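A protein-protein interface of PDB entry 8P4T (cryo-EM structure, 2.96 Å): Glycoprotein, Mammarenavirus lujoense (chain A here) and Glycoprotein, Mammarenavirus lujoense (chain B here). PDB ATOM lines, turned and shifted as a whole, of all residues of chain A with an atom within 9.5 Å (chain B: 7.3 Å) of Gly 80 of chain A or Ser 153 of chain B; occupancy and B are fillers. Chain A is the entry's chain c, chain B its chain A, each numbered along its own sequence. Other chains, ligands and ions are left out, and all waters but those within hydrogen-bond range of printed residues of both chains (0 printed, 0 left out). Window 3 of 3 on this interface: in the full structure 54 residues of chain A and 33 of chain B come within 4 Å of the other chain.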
ATOM      1  N   ILE A  75     -30.445  26.687  23.772  1.00  0.00           N
ATOM      2  CA  ILE A  75     -29.208  26.302  23.102  1.00  0.00           C
ATOM      3  C   ILE A  75     -29.407  25.986  21.629  1.00  0.00           C
ATOM      4  O   ILE A  75     -28.410  25.812  20.912  1.00  0.00           O
ATOM      5  CB  ILE A  75     -28.516  25.120  23.812  1.00  0.00           C
ATOM      6  CG1 ILE A  75     -29.265  23.813  23.569  1.00  0.00           C
ATOM      7  CG2 ILE A  75     -28.404  25.390  25.297  1.00  0.00           C
ATOM      8  CD1 ILE A  75     -28.611  22.637  24.252  1.00  0.00           C
ATOM      9  N   ASN A  76     -30.647  25.904  21.149  1.00  0.00           N
ATOM     10  CA  ASN A  76     -30.887  25.759  19.720  1.00  0.00           C
ATOM     11  C   ASN A  76     -30.857  27.096  18.994  1.00  0.00           C
ATOM     12  O   ASN A  76     -30.974  27.123  17.765  1.00  0.00           O
ATOM     13  CB  ASN A  76     -32.232  25.068  19.477  1.00  0.00           C
ATOM     14  CG  ASN A  76     -32.116  23.558  19.479  1.00  0.00           C
ATOM     15  OD1 ASN A  76     -31.027  23.007  19.332  1.00  0.00           O
ATOM     16  ND2 ASN A  76     -33.245  22.880  19.646  1.00  0.00           N
ATOM     17  N   LEU A  77     -30.700  28.197  19.728  1.00  0.00           N
ATOM     18  CA  LEU A  77     -30.660  29.538  19.165  1.00  0.00           C
ATOM     19  C   LEU A  77     -29.243  30.079  19.043  1.00  0.00           C
ATOM     20  O   LEU A  77     -29.037  31.081  18.350  1.00  0.00           O
ATOM     21  CB  LEU A  77     -31.500  30.500  20.014  1.00  0.00           C
ATOM     22  CG  LEU A  77     -33.020  30.337  19.958  1.00  0.00           C
ATOM     23  CD1 LEU A  77     -33.708  31.526  20.607  1.00  0.00           C
ATOM     24  CD2 LEU A  77     -33.492  30.154  18.527  1.00  0.00           C
ATOM     25  N   LEU A  78     -28.271  29.447  19.698  1.00  0.00           N
ATOM     26  CA  LEU A  78     -26.885  29.891  19.678  1.00  0.00           C
ATOM     27  C   LEU A  78     -26.112  29.361  18.479  1.00  0.00           C
ATOM     28  O   LEU A  78     -24.894  29.554  18.411  1.00  0.00           O
ATOM     29  CB  LEU A  78     -26.179  29.465  20.968  1.00  0.00           C
ATOM     30  CG  LEU A  78     -26.490  30.255  22.236  1.00  0.00           C
ATOM     31  CD1 LEU A  78     -26.022  29.490  23.462  1.00  0.00           C
ATOM     32  CD2 LEU A  78     -25.835  31.620  22.176  1.00  0.00           C
ATOM     33  N   SER A  79     -26.783  28.707  17.535  1.00  0.00           N
ATOM     34  CA  SER A  79     -26.129  28.119  16.373  1.00  0.00           C
ATOM     35  C   SER A  79     -26.227  29.121  15.230  1.00  0.00           C
ATOM     36  O   SER A  79     -27.325  29.424  14.753  1.00  0.00           O
ATOM     37  CB  SER A  79     -26.772  26.785  16.000  1.00  0.00           C
ATOM     38  OG  SER A  79     -28.182  26.898  15.936  1.00  0.00           O
ATOM     39  N   GLY A  80     -25.080  29.635  14.794  1.00  0.00           N
ATOM     40  CA  GLY A  80     -25.062  30.633  13.749  1.00  0.00           C
ATOM     41  C   GLY A  80     -25.487  32.017  14.185  1.00  0.00           C
ATOM     42  O   GLY A  80     -25.720  32.872  13.324  1.00  0.00           O
ATOM     43  N   ARG A  81     -25.603  32.264  15.495  1.00  0.00           N
ATOM     44  CA  ARG A  81     -26.014  33.565  16.012  1.00  0.00           C
ATOM     45  C   ARG A  81     -25.059  34.102  17.073  1.00  0.00           C
ATOM     46  O   ARG A  81     -25.430  35.012  17.820  1.00  0.00           O
ATOM     47  CB  ARG A  81     -27.429  33.499  16.595  1.00  0.00           C
ATOM     48  CG  ARG A  81     -28.553  33.731  15.604  1.00  0.00           C
ATOM     49  CD  ARG A  81     -28.870  32.478  14.813  1.00  0.00           C
ATOM     50  NE  ARG A  81     -30.077  32.641  14.011  1.00  0.00           N
ATOM     51  CZ  ARG A  81     -31.299  32.364  14.439  1.00  0.00           C
ATOM     52  NH1 ARG A  81     -31.515  31.900  15.659  1.00  0.00           N
ATOM     53  NH2 ARG A  81     -32.332  32.557  13.624  1.00  0.00           N
ATOM     54  N   ILE A  82     -23.839  33.570  17.163  1.00  0.00           N
ATOM     55  CA  ILE A  82     -22.923  34.074  18.183  1.00  0.00           C
ATOM     56  C   ILE A  82     -22.342  35.428  17.788  1.00  0.00           C
ATOM     57  O   ILE A  82     -22.017  36.240  18.662  1.00  0.00           O
ATOM     58  CB  ILE A  82     -21.815  33.047  18.474  1.00  0.00           C
ATOM     59  CG1 ILE A  82     -20.972  32.783  17.226  1.00  0.00           C
ATOM     60  CG2 ILE A  82     -22.415  31.755  19.004  1.00  0.00           C
ATOM     61  CD1 ILE A  82     -19.731  31.966  17.502  1.00  0.00           C
ATOM     62  N   ASN A  83     -22.190  35.697  16.488  1.00  0.00           N
ATOM     63  CA  ASN A  83     -21.664  36.986  16.051  1.00  0.00           C
ATOM     64  C   ASN A  83     -22.567  38.142  16.463  1.00  0.00           C
ATOM     65  O   ASN A  83     -22.116  39.293  16.483  1.00  0.00           O
ATOM     66  CB  ASN A  83     -21.467  36.997  14.536  1.00  0.00           C
ATOM     67  CG  ASN A  83     -20.955  35.676  14.008  1.00  0.00           C
ATOM     68  OD1 ASN A  83     -20.070  35.064  14.599  1.00  0.00           O
ATOM     69  ND2 ASN A  83     -21.507  35.231  12.885  1.00  0.00           N
ATOM     70  N   ALA A  84     -23.829  37.859  16.792  1.00  0.00           N
ATOM     71  CA  ALA A  84     -24.712  38.883  17.335  1.00  0.00           C
ATOM     72  C   ALA A  84     -24.343  39.234  18.771  1.00  0.00           C
ATOM     73  O   ALA A  84     -24.418  40.402  19.168  1.00  0.00           O
ATOM     74  CB  ALA A  84     -26.164  38.415  17.252  1.00  0.00           C
ATOM     75  N   ILE A  85     -23.952  38.242  19.565  1.00  0.00           N
ATOM     76  CA  ILE A  85     -23.651  38.467  20.976  1.00  0.00           C
ATOM     77  C   ILE A  85     -22.200  38.883  21.182  1.00  0.00           C
ATOM     78  O   ILE A  85     -21.916  39.828  21.923  1.00  0.00           O
ATOM     79  CB  ILE A  85     -23.992  37.203  21.792  1.00  0.00           C
ATOM     80  CG1 ILE A  85     -25.380  36.686  21.415  1.00  0.00           C
ATOM     81  CG2 ILE A  85     -23.905  37.490  23.280  1.00  0.00           C
ATOM     82  CD1 ILE A  85     -25.585  35.223  21.712  1.00  0.00           C
ATOM     83  N   ILE A  86     -21.261  38.197  20.532  1.00  0.00           N
ATOM     84  CA  ILE A  86     -19.839  38.440  20.733  1.00  0.00           C
ATOM     85  C   ILE A  86     -19.170  38.619  19.378  1.00  0.00           C
ATOM     86  O   ILE A  86     -19.717  38.262  18.333  1.00  0.00           O
ATOM     87  CB  ILE A  86     -19.151  37.304  21.523  1.00  0.00           C
ATOM     88  CG1 ILE A  86     -19.234  35.988  20.751  1.00  0.00           C
ATOM     89  CG2 ILE A  86     -19.765  37.164  22.908  1.00  0.00           C
ATOM     90  CD1 ILE A  86     -18.225  34.957  21.199  1.00  0.00           C
ATOM     91  N   ASP A  88     -16.965  37.719  16.441  1.00  0.00           N
ATOM     92  CA  ASP A  88     -16.396  36.527  15.819  1.00  0.00           C
ATOM     93  C   ASP A  88     -14.893  36.670  15.616  1.00  0.00           C
ATOM     94  O   ASP A  88     -14.145  35.692  15.753  1.00  0.00           O
ATOM     95  CB  ASP A  88     -17.091  36.245  14.488  1.00  0.00           C
ATOM     96  CG  ASP A  88     -17.053  37.432  13.546  1.00  0.00           C
ATOM     97  OD1 ASP A  88     -17.388  38.552  13.986  1.00  0.00           O
ATOM     98  OD2 ASP A  88     -16.687  37.246  12.367  1.00  0.00           O
ATOM     99  N   MET A  92     -12.101  33.883  16.814  1.00  0.00           N
ATOM    100  CA  MET A  92     -11.300  33.191  15.811  1.00  0.00           C
ATOM    101  C   MET A  92      -9.822  33.538  15.926  1.00  0.00           C
ATOM    102  O   MET A  92      -8.969  32.681  15.670  1.00  0.00           O
ATOM    103  CB  MET A  92     -11.823  33.516  14.414  1.00  0.00           C
ATOM    104  CG  MET A  92     -13.189  32.918  14.130  1.00  0.00           C
ATOM    105  SD  MET A  92     -14.087  33.829  12.867  1.00  0.00           S
ATOM    106  CE  MET A  92     -12.959  33.651  11.494  1.00  0.00           C
ATOM    107  N   GLU B  71     -24.156  19.786  18.212  1.00  0.00           N
ATOM    108  CA  GLU B  71     -23.049  20.569  17.670  1.00  0.00           C
ATOM    109  C   GLU B  71     -21.780  19.730  17.550  1.00  0.00           C
ATOM    110  O   GLU B  71     -21.057  19.829  16.551  1.00  0.00           O
ATOM    111  CB  GLU B  71     -22.808  21.803  18.537  1.00  0.00           C
ATOM    112  CG  GLU B  71     -23.924  22.824  18.445  1.00  0.00           C
ATOM    113  CD  GLU B  71     -23.959  23.525  17.103  1.00  0.00           C
ATOM    114  OE1 GLU B  71     -22.882  23.720  16.501  1.00  0.00           O
ATOM    115  OE2 GLU B  71     -25.066  23.870  16.642  1.00  0.00           O
ATOM    116  N   ARG B 147     -16.308  28.266  20.318  1.00  0.00           N
ATOM    117  CA  ARG B 147     -15.371  27.834  19.285  1.00  0.00           C
ATOM    118  C   ARG B 147     -15.970  26.724  18.435  1.00  0.00           C
ATOM    119  O   ARG B 147     -15.808  26.714  17.209  1.00  0.00           O
ATOM    120  CB  ARG B 147     -14.064  27.363  19.920  1.00  0.00           C
ATOM    121  CG  ARG B 147     -13.197  28.465  20.493  1.00  0.00           C
ATOM    122  CD  ARG B 147     -11.818  27.925  20.826  1.00  0.00           C
ATOM    123  NE  ARG B 147     -11.320  27.046  19.776  1.00  0.00           N
ATOM    124  CZ  ARG B 147     -10.643  25.926  19.992  1.00  0.00           C
ATOM    125  NH1 ARG B 147     -10.366  25.511  21.216  1.00  0.00           N
ATOM    126  NH2 ARG B 147     -10.232  25.206  18.952  1.00  0.00           N
ATOM    127  N   LEU B 148     -16.663  25.778  19.073  1.00  0.00           N
ATOM    128  CA  LEU B 148     -17.321  24.705  18.334  1.00  0.00           C
ATOM    129  C   LEU B 148     -18.370  25.263  17.382  1.00  0.00           C
ATOM    130  O   LEU B 148     -18.446  24.853  16.218  1.00  0.00           O
ATOM    131  CB  LEU B 148     -17.954  23.716  19.313  1.00  0.00           C
ATOM    132  CG  LEU B 148     -18.416  22.366  18.767  1.00  0.00           C
ATOM    133  CD1 LEU B 148     -17.223  21.475  18.486  1.00  0.00           C
ATOM    134  CD2 LEU B 148     -19.362  21.698  19.749  1.00  0.00           C
ATOM    135  N   LEU B 149     -19.177  26.215  17.858  1.00  0.00           N
ATOM    136  CA  LEU B 149     -20.219  26.795  17.016  1.00  0.00           C
ATOM    137  C   LEU B 149     -19.614  27.542  15.834  1.00  0.00           C
ATOM    138  O   LEU B 149     -20.103  27.435  14.703  1.00  0.00           O
ATOM    139  CB  LEU B 149     -21.100  27.735  17.839  1.00  0.00           C
ATOM    140  CG  LEU B 149     -21.968  27.143  18.949  1.00  0.00           C
ATOM    141  CD1 LEU B 149     -22.223  28.185  20.022  1.00  0.00           C
ATOM    142  CD2 LEU B 149     -23.279  26.635  18.384  1.00  0.00           C
ATOM    143  N   LYS B 150     -18.536  28.293  16.074  1.00  0.00           N
ATOM    144  CA  LYS B 150     -17.918  29.055  14.997  1.00  0.00           C
ATOM    145  C   LYS B 150     -17.255  28.135  13.977  1.00  0.00           C
ATOM    146  O   LYS B 150     -17.343  28.377  12.766  1.00  0.00           O
ATOM    147  CB  LYS B 150     -16.906  30.043  15.576  1.00  0.00           C
ATOM    148  CG  LYS B 150     -16.210  30.914  14.546  1.00  0.00           C
ATOM    149  CD  LYS B 150     -17.198  31.584  13.610  1.00  0.00           C
ATOM    150  CE  LYS B 150     -18.036  32.623  14.321  1.00  0.00           C
ATOM    151  NZ  LYS B 150     -19.007  33.254  13.388  1.00  0.00           N
ATOM    152  N   GLU B 151     -16.596  27.072  14.445  1.00  0.00           N
ATOM    153  CA  GLU B 151     -16.008  26.104  13.525  1.00  0.00           C
ATOM    154  C   GLU B 151     -17.083  25.400  12.710  1.00  0.00           C
ATOM    155  O   GLU B 151     -16.880  25.102  11.527  1.00  0.00           O
ATOM    156  CB  GLU B 151     -15.161  25.092  14.295  1.00  0.00           C
ATOM    157  CG  GLU B 151     -13.850  25.658  14.810  1.00  0.00           C
ATOM    158  CD  GLU B 151     -12.881  24.581  15.242  1.00  0.00           C
ATOM    159  OE1 GLU B 151     -13.224  23.388  15.117  1.00  0.00           O
ATOM    160  OE2 GLU B 151     -11.774  24.926  15.706  1.00  0.00           O
ATOM    161  N   ASN B 152     -18.233  25.117  13.326  1.00  0.00           N
ATOM    162  CA  ASN B 152     -19.317  24.473  12.595  1.00  0.00           C
ATOM    163  C   ASN B 152     -19.898  25.406  11.544  1.00  0.00           C
ATOM    164  O   ASN B 152     -20.242  24.971  10.440  1.00  0.00           O
ATOM    165  CB  ASN B 152     -20.407  24.017  13.564  1.00  0.00           C
ATOM    166  CG  ASN B 152     -20.206  22.598  14.039  1.00  0.00           C
ATOM    167  OD1 ASN B 152     -19.656  21.766  13.320  1.00  0.00           O
ATOM    168  ND2 ASN B 152     -20.653  22.309  15.255  1.00  0.00           N
ATOM    169  N   SER B 153     -20.018  26.694  11.870  1.00  0.00           N
ATOM    170  CA  SER B 153     -20.622  27.634  10.932  1.00  0.00           C
ATOM    171  C   SER B 153     -19.685  27.951   9.771  1.00  0.00           C
ATOM    172  O   SER B 153     -20.131  28.071   8.625  1.00  0.00           O
ATOM    173  CB  SER B 153     -21.021  28.918  11.661  1.00  0.00           C
ATOM    174  OG  SER B 153     -22.019  28.662  12.632  1.00  0.00           O
ATOM    175  N   GLU B 154     -18.387  28.087  10.043  1.00  0.00           N
ATOM    176  CA  GLU B 154     -17.448  28.498   9.004  1.00  0.00           C
ATOM    177  C   GLU B 154     -16.830  27.341   8.228  1.00  0.00           C
ATOM    178  O   GLU B 154     -16.693  27.429   7.003  1.00  0.00           O
ATOM    179  CB  GLU B 154     -16.332  29.349   9.613  1.00  0.00           C
ATOM    180  CG  GLU B 154     -16.819  30.629  10.258  1.00  0.00           C
ATOM    181  CD  GLU B 154     -17.406  31.601   9.255  1.00  0.00           C
ATOM    182  OE1 GLU B 154     -16.883  31.679   8.124  1.00  0.00           O
ATOM    183  OE2 GLU B 154     -18.392  32.287   9.597  1.00  0.00           O
ATOM    184  N   THR B 155     -16.449  26.258   8.899  1.00  0.00           N
ATOM    185  CA  THR B 155     -15.663  25.199   8.277  1.00  0.00           C
ATOM    186  C   THR B 155     -16.457  23.892   8.223  1.00  0.00           C
ATOM    187  O   THR B 155     -15.926  22.800   8.437  1.00  0.00           O
ATOM    188  CB  THR B 155     -14.334  25.033   9.017  1.00  0.00           C
ATOM    189  OG1 THR B 155     -13.706  26.314   9.132  1.00  0.00           O
ATOM    190  CG2 THR B 155     -13.369  24.156   8.230  1.00  0.00           C
ATOM    191  N   HIS B 156     -17.763  23.990   7.964  1.00  0.00           N
ATOM    192  CA  HIS B 156     -18.560  22.779   7.786  1.00  0.00           C
ATOM    193  C   HIS B 156     -18.177  22.026   6.517  1.00  0.00           C
ATOM    194  O   HIS B 156     -18.271  20.794   6.479  1.00  0.00           O
ATOM    195  CB  HIS B 156     -20.048  23.117   7.762  1.00  0.00           C
ATOM    196  CG  HIS B 156     -20.931  21.917   7.609  1.00  0.00           C
ATOM    197  ND1 HIS B 156     -21.864  21.804   6.601  1.00  0.00           N
ATOM    198  CD2 HIS B 156     -21.013  20.773   8.329  1.00  0.00           C
ATOM    199  CE1 HIS B 156     -22.489  20.644   6.712  1.00  0.00           C
ATOM    200  NE2 HIS B 156     -21.991  20.000   7.752  1.00  0.00           N
ATOM    201  N   TYR B 157     -17.772  22.742   5.467  1.00  0.00           N
ATOM    202  CA  TYR B 157     -17.430  22.090   4.205  1.00  0.00           C
ATOM    203  C   TYR B 157     -16.249  21.138   4.369  1.00  0.00           C
ATOM    204  O   TYR B 157     -16.293  19.993   3.905  1.00  0.00           O
ATOM    205  CB  TYR B 157     -17.149  23.140   3.126  1.00  0.00           C
ATOM    206  CG  TYR B 157     -15.951  24.028   3.383  1.00  0.00           C
ATOM    207  CD1 TYR B 157     -16.019  25.078   4.288  1.00  0.00           C
ATOM    208  CD2 TYR B 157     -14.755  23.822   2.709  1.00  0.00           C
ATOM    209  CE1 TYR B 157     -14.928  25.891   4.520  1.00  0.00           C
ATOM    210  CE2 TYR B 157     -13.659  24.630   2.935  1.00  0.00           C
ATOM    211  CZ  TYR B 157     -13.751  25.663   3.841  1.00  0.00           C
ATOM    212  OH  TYR B 157     -12.663  26.471   4.068  1.00  0.00           O
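Hydrophobic or aromatic side chains of chain A that line the printed part of chain B: Ile 82 and Met 92.
Of the 12 printed residues of chain B, 4 touch a printed residue of chain A.
Among the printed residues, 9 pairs touch across the chains.
Among the printed residues, no Asp or Glu carboxylate lies within 4 Å of a Lys or Arg side-chain nitrogen of the other chain.
The side-chain amide nitrogen (ND2) of Asn 152 of chain B sits at hydrogen-bond distance from the backbone carbonyl oxygen (O) of Glu 71 of chain B.
The backbone carbonyl oxygen of Leu 149 of chain B lies within hydrogen-bond range of the side-chain hydroxyl of Ser 153 of chain B (3.1 Å).
The side-chain amino group (NZ) of Lys 150 of chain B lies within salt-bridge range of the side-chain carboxylate (OE2) of Glu 154 of chain B, at 3.96 Å.
The backbone carbonyl oxygen (O) of Asn 76 of chain A sits at hydrogen-bond distance from the side-chain hydroxyl (OG) of Ser 79 of chain A (3.3 Å).
Among the printed residues, pairs that only touch across the chains: Leu 78 of chain A with Leu 149 of chain B (3.3 Å), Ser 79 of chain A with Glu 71 of chain B (3.4 Å), Met 92 of chain A with Lys 150 of chain B (3.6 Å), Ile 82 of chain A with Lys 150 of chain B (3.7 Å), Ile 82 of chain A with Leu 149 of chain B (3.7 Å), Asp 88 of chain A with Lys 150 of chain B (3.7 Å), Ser 79 of chain A with Leu 149 of chain B (3.8 Å) and Gly 80 of chain A with Ser 153 of chain B (3.8 Å).
NZ of Lys 150 of chain B is in hydrogen-bond range of OD1 of Asn 83 of chain A (2.4 Å).
Gly 80 of chain A touches just one residue of chain B: Ser 153 (3.8 Å).
Of the printed residues of chain A, Ser 153 of chain B touches Gly 80 (3.8 Å).
No residue of chain A comes within 4 Å of Glu 154 of chain B.
Printed residues of chain A within 4 Å of Lys 150 of chain B: Ile 82 (3.7 Å), Asn 83 (2.4 Å), Asp 88 (3.7 Å) and Met 92 (3.6 Å).
Of the printed residues of chain B, Leu 78 of chain A touches Leu 149.
Of the printed residues of chain A, Leu 149 of chain B touches Leu 78 (3.3 Å), Ser 79 (3.8 Å) and Ile 82 (3.7 Å).
Of the printed residues of chain B, Met 92 of chain A touches Lys 150.
Tyr 157 of chain B touches none of the printed residues of chain A.
The nearest residue of chain B that does not touch Gly 80 of chain A is Leu 149 of chain B (5.0 Å).
The nearest printed residue of chain A that does not touch Leu 149 of chain B is Gly 80 of chain A (5.0 Å).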
